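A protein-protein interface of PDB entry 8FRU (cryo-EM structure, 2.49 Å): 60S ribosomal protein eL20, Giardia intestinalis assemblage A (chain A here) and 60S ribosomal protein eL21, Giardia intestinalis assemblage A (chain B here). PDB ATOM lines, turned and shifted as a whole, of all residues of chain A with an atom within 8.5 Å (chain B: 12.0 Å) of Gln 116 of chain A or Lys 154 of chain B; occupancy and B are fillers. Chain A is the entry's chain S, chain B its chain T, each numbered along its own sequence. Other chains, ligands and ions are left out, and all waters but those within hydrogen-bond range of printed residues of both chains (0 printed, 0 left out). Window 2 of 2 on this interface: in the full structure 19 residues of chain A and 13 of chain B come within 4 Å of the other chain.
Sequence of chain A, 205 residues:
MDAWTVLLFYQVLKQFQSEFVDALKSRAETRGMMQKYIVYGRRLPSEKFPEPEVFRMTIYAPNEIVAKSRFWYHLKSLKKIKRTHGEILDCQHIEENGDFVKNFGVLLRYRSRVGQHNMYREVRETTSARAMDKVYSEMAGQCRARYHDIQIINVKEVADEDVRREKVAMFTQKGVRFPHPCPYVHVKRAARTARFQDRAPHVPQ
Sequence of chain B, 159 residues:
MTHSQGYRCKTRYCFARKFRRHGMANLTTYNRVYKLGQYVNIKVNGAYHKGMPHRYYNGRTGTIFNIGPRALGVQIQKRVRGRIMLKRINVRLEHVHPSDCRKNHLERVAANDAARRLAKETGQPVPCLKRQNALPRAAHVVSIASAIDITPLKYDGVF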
ATOM      1  N   TYR A  73      14.766   5.482  -6.155  1.00  0.00           N
ATOM      2  CA  TYR A  73      15.566   5.744  -7.343  1.00  0.00           C
ATOM      3  C   TYR A  73      15.990   7.204  -7.407  1.00  0.00           C
ATOM      4  O   TYR A  73      17.149   7.511  -7.698  1.00  0.00           O
ATOM      5  CB  TYR A  73      14.776   5.356  -8.593  1.00  0.00           C
ATOM      6  CG  TYR A  73      15.446   5.740  -9.888  1.00  0.00           C
ATOM      7  CD1 TYR A  73      15.230   6.980 -10.462  1.00  0.00           C
ATOM      8  CD2 TYR A  73      16.297   4.863 -10.534  1.00  0.00           C
ATOM      9  CE1 TYR A  73      15.842   7.334 -11.638  1.00  0.00           C
ATOM     10  CE2 TYR A  73      16.910   5.207 -11.711  1.00  0.00           C
ATOM     11  CZ  TYR A  73      16.678   6.442 -12.260  1.00  0.00           C
ATOM     12  OH  TYR A  73      17.292   6.786 -13.437  1.00  0.00           O
ATOM     13  N   LEU A 107       6.720  18.441 -18.282  1.00  0.00           N
ATOM     14  CA  LEU A 107       8.124  18.559 -18.642  1.00  0.00           C
ATOM     15  C   LEU A 107       8.841  17.288 -18.222  1.00  0.00           C
ATOM     16  O   LEU A 107       8.699  16.841 -17.080  1.00  0.00           O
ATOM     17  CB  LEU A 107       8.757  19.781 -17.980  1.00  0.00           C
ATOM     18  CG  LEU A 107      10.163  20.144 -18.436  1.00  0.00           C
ATOM     19  CD1 LEU A 107      10.135  20.666 -19.855  1.00  0.00           C
ATOM     20  CD2 LEU A 107      10.778  21.158 -17.497  1.00  0.00           C
ATOM     21  N   LEU A 108       9.606  16.705 -19.138  1.00  0.00           N
ATOM     22  CA  LEU A 108      10.198  15.401 -18.890  1.00  0.00           C
ATOM     23  C   LEU A 108      11.533  15.296 -19.606  1.00  0.00           C
ATOM     24  O   LEU A 108      11.862  16.103 -20.474  1.00  0.00           O
ATOM     25  CB  LEU A 108       9.266  14.274 -19.338  1.00  0.00           C
ATOM     26  CG  LEU A 108       8.904  14.246 -20.820  1.00  0.00           C
ATOM     27  CD1 LEU A 108       9.646  13.138 -21.532  1.00  0.00           C
ATOM     28  CD2 LEU A 108       7.415  14.079 -20.998  1.00  0.00           C
ATOM     29  N   ARG A 109      12.310  14.298 -19.206  1.00  0.00           N
ATOM     30  CA  ARG A 109      13.513  13.904 -19.918  1.00  0.00           C
ATOM     31  C   ARG A 109      13.481  12.401 -20.128  1.00  0.00           C
ATOM     32  O   ARG A 109      13.087  11.649 -19.237  1.00  0.00           O
ATOM     33  CB  ARG A 109      14.779  14.298 -19.165  1.00  0.00           C
ATOM     34  CG  ARG A 109      14.750  13.968 -17.696  1.00  0.00           C
ATOM     35  CD  ARG A 109      16.034  14.383 -17.027  1.00  0.00           C
ATOM     36  NE  ARG A 109      17.135  13.481 -17.335  1.00  0.00           N
ATOM     37  CZ  ARG A 109      18.316  13.519 -16.736  1.00  0.00           C
ATOM     38  NH1 ARG A 109      18.585  14.408 -15.797  1.00  0.00           N
ATOM     39  NH2 ARG A 109      19.252  12.643 -17.087  1.00  0.00           N
ATOM     40  N   TYR A 110      13.887  11.967 -21.314  1.00  0.00           N
ATOM     41  CA  TYR A 110      13.891  10.554 -21.640  1.00  0.00           C
ATOM     42  C   TYR A 110      15.182  10.219 -22.365  1.00  0.00           C
ATOM     43  O   TYR A 110      15.823  11.080 -22.966  1.00  0.00           O
ATOM     44  CB  TYR A 110      12.676  10.167 -22.490  1.00  0.00           C
ATOM     45  CG  TYR A 110      12.768  10.591 -23.935  1.00  0.00           C
ATOM     46  CD1 TYR A 110      12.704  11.928 -24.293  1.00  0.00           C
ATOM     47  CD2 TYR A 110      12.915   9.651 -24.942  1.00  0.00           C
ATOM     48  CE1 TYR A 110      12.791  12.313 -25.608  1.00  0.00           C
ATOM     49  CE2 TYR A 110      13.000  10.025 -26.257  1.00  0.00           C
ATOM     50  CZ  TYR A 110      12.938  11.354 -26.587  1.00  0.00           C
ATOM     51  OH  TYR A 110      13.023  11.725 -27.908  1.00  0.00           O
ATOM     52  N   ARG A 111      15.565   8.953 -22.287  1.00  0.00           N
ATOM     53  CA  ARG A 111      16.756   8.460 -22.958  1.00  0.00           C
ATOM     54  C   ARG A 111      16.366   7.694 -24.210  1.00  0.00           C
ATOM     55  O   ARG A 111      15.518   6.801 -24.161  1.00  0.00           O
ATOM     56  CB  ARG A 111      17.585   7.574 -22.036  1.00  0.00           C
ATOM     57  CG  ARG A 111      18.794   6.990 -22.726  1.00  0.00           C
ATOM     58  CD  ARG A 111      19.311   5.789 -21.993  1.00  0.00           C
ATOM     59  NE  ARG A 111      19.517   6.102 -20.586  1.00  0.00           N
ATOM     60  CZ  ARG A 111      20.623   6.653 -20.108  1.00  0.00           C
ATOM     61  NH1 ARG A 111      21.640   6.951 -20.898  1.00  0.00           N
ATOM     62  NH2 ARG A 111      20.710   6.912 -18.809  1.00  0.00           N
ATOM     63  N   SER A 112      16.974   8.055 -25.323  1.00  0.00           N
ATOM     64  CA  SER A 112      16.775   7.354 -26.572  1.00  0.00           C
ATOM     65  C   SER A 112      17.925   6.381 -26.791  1.00  0.00           C
ATOM     66  O   SER A 112      18.663   6.028 -25.870  1.00  0.00           O
ATOM     67  CB  SER A 112      16.656   8.348 -27.725  1.00  0.00           C
ATOM     68  OG  SER A 112      17.883   9.015 -27.944  1.00  0.00           O
ATOM     69  N   ARG A 113      18.084   5.945 -28.029  1.00  0.00           N
ATOM     70  CA  ARG A 113      19.181   5.075 -28.416  1.00  0.00           C
ATOM     71  C   ARG A 113      20.471   5.839 -28.681  1.00  0.00           C
ATOM     72  O   ARG A 113      21.489   5.215 -28.991  1.00  0.00           O
ATOM     73  CB  ARG A 113      18.746   4.259 -29.635  1.00  0.00           C
ATOM     74  CG  ARG A 113      19.630   3.097 -30.005  1.00  0.00           C
ATOM     75  CD  ARG A 113      19.383   2.697 -31.454  1.00  0.00           C
ATOM     76  NE  ARG A 113      18.934   3.817 -32.269  1.00  0.00           N
ATOM     77  CZ  ARG A 113      19.712   4.505 -33.091  1.00  0.00           C
ATOM     78  NH1 ARG A 113      20.988   4.198 -33.252  1.00  0.00           N
ATOM     79  NH2 ARG A 113      19.195   5.522 -33.775  1.00  0.00           N
ATOM     80  N   VAL A 114      20.458   7.167 -28.549  1.00  0.00           N
ATOM     81  CA  VAL A 114      21.603   8.005 -28.892  1.00  0.00           C
ATOM     82  C   VAL A 114      21.809   9.084 -27.835  1.00  0.00           C
ATOM     83  O   VAL A 114      22.330  10.163 -28.131  1.00  0.00           O
ATOM     84  CB  VAL A 114      21.412   8.641 -30.283  1.00  0.00           C
ATOM     85  CG1 VAL A 114      22.692   9.298 -30.756  1.00  0.00           C
ATOM     86  CG2 VAL A 114      20.937   7.604 -31.285  1.00  0.00           C
ATOM     87  N   GLY A 115      21.423   8.805 -26.599  1.00  0.00           N
ATOM     88  CA  GLY A 115      21.551   9.767 -25.524  1.00  0.00           C
ATOM     89  C   GLY A 115      20.220  10.206 -24.950  1.00  0.00           C
ATOM     90  O   GLY A 115      19.205   9.515 -25.044  1.00  0.00           O
ATOM     91  N   GLN A 116      20.232  11.393 -24.345  1.00  0.00           N
ATOM     92  CA  GLN A 116      19.098  11.878 -23.575  1.00  0.00           C
ATOM     93  C   GLN A 116      18.628  13.228 -24.094  1.00  0.00           C
ATOM     94  O   GLN A 116      19.404  14.014 -24.638  1.00  0.00           O
ATOM     95  CB  GLN A 116      19.443  11.983 -22.092  1.00  0.00           C
ATOM     96  CG  GLN A 116      20.053  10.719 -21.535  1.00  0.00           C
ATOM     97  CD  GLN A 116      20.382  10.841 -20.072  1.00  0.00           C
ATOM     98  OE1 GLN A 116      19.495  11.026 -19.244  1.00  0.00           O
ATOM     99  NE2 GLN A 116      21.661  10.736 -19.740  1.00  0.00           N
ATOM    100  N   HIS A 117      17.337  13.493 -23.896  1.00  0.00           N
ATOM    101  CA  HIS A 117      16.698  14.681 -24.436  1.00  0.00           C
ATOM    102  C   HIS A 117      15.643  15.186 -23.466  1.00  0.00           C
ATOM    103  O   HIS A 117      15.026  14.408 -22.737  1.00  0.00           O
ATOM    104  CB  HIS A 117      16.046  14.397 -25.794  1.00  0.00           C
ATOM    105  CG  HIS A 117      16.842  13.482 -26.669  1.00  0.00           C
ATOM    106  ND1 HIS A 117      17.956  13.899 -27.363  1.00  0.00           N
ATOM    107  CD2 HIS A 117      16.688  12.170 -26.959  1.00  0.00           C
ATOM    108  CE1 HIS A 117      18.454  12.883 -28.044  1.00  0.00           C
ATOM    109  NE2 HIS A 117      17.702  11.822 -27.816  1.00  0.00           N
ATOM    110  N   ASN A 118      15.436  16.497 -23.473  1.00  0.00           N
ATOM    111  CA  ASN A 118      14.347  17.124 -22.743  1.00  0.00           C
ATOM    112  C   ASN A 118      13.147  17.307 -23.660  1.00  0.00           C
ATOM    113  O   ASN A 118      13.271  17.323 -24.884  1.00  0.00           O
ATOM    114  CB  ASN A 118      14.779  18.471 -22.177  1.00  0.00           C
ATOM    115  CG  ASN A 118      15.876  18.343 -21.153  1.00  0.00           C
ATOM    116  OD1 ASN A 118      15.664  17.815 -20.066  1.00  0.00           O
ATOM    117  ND2 ASN A 118      17.062  18.816 -21.498  1.00  0.00           N
ATOM    118  N   MET A 119      11.975  17.453 -23.054  1.00  0.00           N
ATOM    119  CA  MET A 119      10.754  17.480 -23.842  1.00  0.00           C
ATOM    120  C   MET A 119       9.626  18.103 -23.038  1.00  0.00           C
ATOM    121  O   MET A 119       9.426  17.765 -21.872  1.00  0.00           O
ATOM    122  CB  MET A 119      10.360  16.069 -24.281  1.00  0.00           C
ATOM    123  CG  MET A 119       9.275  16.014 -25.326  1.00  0.00           C
ATOM    124  SD  MET A 119       9.434  14.545 -26.347  1.00  0.00           S
ATOM    125  CE  MET A 119       7.942  14.658 -27.312  1.00  0.00           C
ATOM    126  N   ASP A 149      12.316   4.426 -18.655  1.00  0.00           N
ATOM    127  CA  ASP A 149      13.208   5.232 -19.472  1.00  0.00           C
ATOM    128  C   ASP A 149      12.875   6.716 -19.411  1.00  0.00           C
ATOM    129  O   ASP A 149      13.489   7.505 -20.132  1.00  0.00           O
ATOM    130  CB  ASP A 149      13.159   4.760 -20.923  1.00  0.00           C
ATOM    131  CG  ASP A 149      13.047   3.258 -21.046  1.00  0.00           C
ATOM    132  OD1 ASP A 149      13.631   2.541 -20.210  1.00  0.00           O
ATOM    133  OD2 ASP A 149      12.376   2.785 -21.985  1.00  0.00           O
ATOM    134  N   GLN A 151      11.750  10.308 -17.028  1.00  0.00           N
ATOM    135  CA  GLN A 151      11.763  11.016 -15.754  1.00  0.00           C
ATOM    136  C   GLN A 151      10.845  12.221 -15.866  1.00  0.00           C
ATOM    137  O   GLN A 151      11.066  13.089 -16.713  1.00  0.00           O
ATOM    138  CB  GLN A 151      13.178  11.459 -15.383  1.00  0.00           C
ATOM    139  CG  GLN A 151      14.068  10.358 -14.868  1.00  0.00           C
ATOM    140  CD  GLN A 151      15.441  10.858 -14.498  1.00  0.00           C
ATOM    141  OE1 GLN A 151      15.583  11.808 -13.735  1.00  0.00           O
ATOM    142  NE2 GLN A 151      16.467  10.219 -15.040  1.00  0.00           N
ATOM    143  N   ILE A 153       9.715  15.650 -14.704  1.00  0.00           N
ATOM    144  CA  ILE A 153      10.303  16.744 -13.944  1.00  0.00           C
ATOM    145  C   ILE A 153       9.230  17.510 -13.186  1.00  0.00           C
ATOM    146  O   ILE A 153       9.347  17.739 -11.979  1.00  0.00           O
ATOM    147  CB  ILE A 153      11.104  17.672 -14.874  1.00  0.00           C
ATOM    148  CG1 ILE A 153      12.051  16.866 -15.756  1.00  0.00           C
ATOM    149  CG2 ILE A 153      11.881  18.681 -14.063  1.00  0.00           C
ATOM    150  CD1 ILE A 153      13.269  16.398 -15.049  1.00  0.00           C
ATOM    151  N   ILE B 150      12.771  17.363  -6.205  1.00  0.00           N
ATOM    152  CA  ILE B 150      12.361  17.310  -7.601  1.00  0.00           C
ATOM    153  C   ILE B 150      13.507  16.748  -8.435  1.00  0.00           C
ATOM    154  O   ILE B 150      14.644  16.633  -7.979  1.00  0.00           O
ATOM    155  CB  ILE B 150      11.933  18.695  -8.129  1.00  0.00           C
ATOM    156  CG1 ILE B 150      11.131  18.559  -9.421  1.00  0.00           C
ATOM    157  CG2 ILE B 150      13.143  19.588  -8.329  1.00  0.00           C
ATOM    158  CD1 ILE B 150       9.638  18.577  -9.211  1.00  0.00           C
ATOM    159  N   THR B 151      13.191  16.410  -9.671  1.00  0.00           N
ATOM    160  CA  THR B 151      14.090  15.818 -10.652  1.00  0.00           C
ATOM    161  C   THR B 151      14.672  16.896 -11.553  1.00  0.00           C
ATOM    162  O   THR B 151      13.920  17.743 -12.050  1.00  0.00           O
ATOM    163  CB  THR B 151      13.339  14.792 -11.491  1.00  0.00           C
ATOM    164  OG1 THR B 151      12.362  14.141 -10.674  1.00  0.00           O
ATOM    165  CG2 THR B 151      14.281  13.768 -12.028  1.00  0.00           C
ATOM    166  N   PRO B 152      15.983  16.924 -11.774  1.00  0.00           N
ATOM    167  CA  PRO B 152      16.577  18.002 -12.577  1.00  0.00           C
ATOM    168  C   PRO B 152      16.510  17.715 -14.072  1.00  0.00           C
ATOM    169  O   PRO B 152      16.248  16.602 -14.524  1.00  0.00           O
ATOM    170  CB  PRO B 152      18.025  18.057 -12.083  1.00  0.00           C
ATOM    171  N   LEU B 153      16.769  18.764 -14.848  1.00  0.00           N
ATOM    172  CA  LEU B 153      16.831  18.666 -16.296  1.00  0.00           C
ATOM    173  C   LEU B 153      18.141  18.002 -16.710  1.00  0.00           C
ATOM    174  O   LEU B 153      19.061  17.833 -15.909  1.00  0.00           O
ATOM    175  CB  LEU B 153      16.690  20.054 -16.920  1.00  0.00           C
ATOM    176  CG  LEU B 153      15.259  20.552 -17.146  1.00  0.00           C
ATOM    177  CD1 LEU B 153      14.729  21.244 -15.904  1.00  0.00           C
ATOM    178  CD2 LEU B 153      15.185  21.492 -18.334  1.00  0.00           C
ATOM    179  N   LYS B 154      18.236  17.625 -17.980  1.00  0.00           N
ATOM    180  CA  LYS B 154      19.423  16.942 -18.485  1.00  0.00           C
ATOM    181  C   LYS B 154      20.541  17.922 -18.831  1.00  0.00           C
ATOM    182  O   LYS B 154      20.356  18.844 -19.622  1.00  0.00           O
ATOM    183  CB  LYS B 154      19.059  16.089 -19.704  1.00  0.00           C
ATOM    184  CG  LYS B 154      20.233  15.647 -20.560  1.00  0.00           C
ATOM    185  CD  LYS B 154      21.288  14.937 -19.737  1.00  0.00           C
ATOM    186  CE  LYS B 154      22.395  14.398 -20.610  1.00  0.00           C
ATOM    187  NZ  LYS B 154      22.649  15.278 -21.769  1.00  0.00           N
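The guanidinium group (NH2) of Arg 109 of chain A sits at hydrogen-bond distance from the side-chain amide oxygen (OE1) of Gln 116 of chain A, at 2.7 Å. The backbone carbonyl oxygen (O) of Leu 107 of chain A is in hydrogen-bond range of the backbone NH (N) of Ile 153 of chain A (2.8 Å). The backbone carbonyl oxygen of Arg 109 of chain A is in hydrogen-bond range of the backbone NH of Gln 151 of chain A, at 2.9 Å.
Among the printed residues, merely in contact across the chains: Arg 109 of chain A with Lys 154 of chain B, Gln 116 of chain A with Lys 154 of chain B, Asn 118 of chain A with Leu 153 of chain B, Gln 151 of chain A with Thr 151 of chain B, Ile 153 of chain A with Ile 150 of chain B, Ile 153 of chain A with Thr 151 of chain B and Ile 153 of chain A with Pro 152 of chain B.
NH1 of Arg 109 of chain A lies within hydrogen-bond range of O of Leu 153 of chain B, 3.5 Å away. The backbone NH (N) of Lys 154 of chain B is in hydrogen-bond range of the side-chain amide oxygen (OD1) of Asn 118 of chain A (3.3 Å). The guanidinium group (NH1) of Arg 109 of chain A lies close to the backbone carbonyl oxygen (O) of Pro 152 of chain B (3.4 Å).
Gln 116 of chain A touches just one residue of chain B: Lys 154 (3.8 Å). Of chain A, only Arg 109, Gln 116 and Asn 118 come within 4 Å of Lys 154 of chain B. Arg 109 of chain A touches just these residues of chain B: Pro 152, Leu 153 and Lys 154. No residue of chain B comes within 4 Å of Tyr 110 of chain A. No residue of chain B comes within 4 Å of Arg 111 of chain A. No residue of chain B comes within 4 Å of Ser 112 of chain A. No residue of chain B comes within 4 Å of His 117 of chain A. Of the printed residues of chain A, Pro 152 of chain B touches Arg 109 and Ile 153. Of the printed residues of chain A, Thr 151 of chain B touches Gln 151 (2.9 Å) and Ile 153 (3.0 Å). Of the printed residues of chain B, Ile 153 of chain A touches Ile 150, Thr 151 and Pro 152. Of the printed residues of chain A, Ile 150 of chain B touches Ile 153 (2.9 Å). Leu 108 of chain A touches none of the printed residues of chain B. The nearest residue of chain B that does not touch Gln 116 of chain A is Leu 153 of chain B (7.5 Å). The nearest printed residue of chain A that does not touch Pro 152 of chain B is Gln 151 of chain A (4.9 Å).
Of the 17 printed residues of chain A, 5 touch a printed residue of chain B. Printed residues of chain A that touch a printed residue of chain B: Arg 109, Gln 116, Asn 118, Gln 151 and Ile 153. Hydrophobic or aromatic side chains of chain A that line the printed part of chain B: Ile 153. Among the printed residues, 10 pairs touch across the chains.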
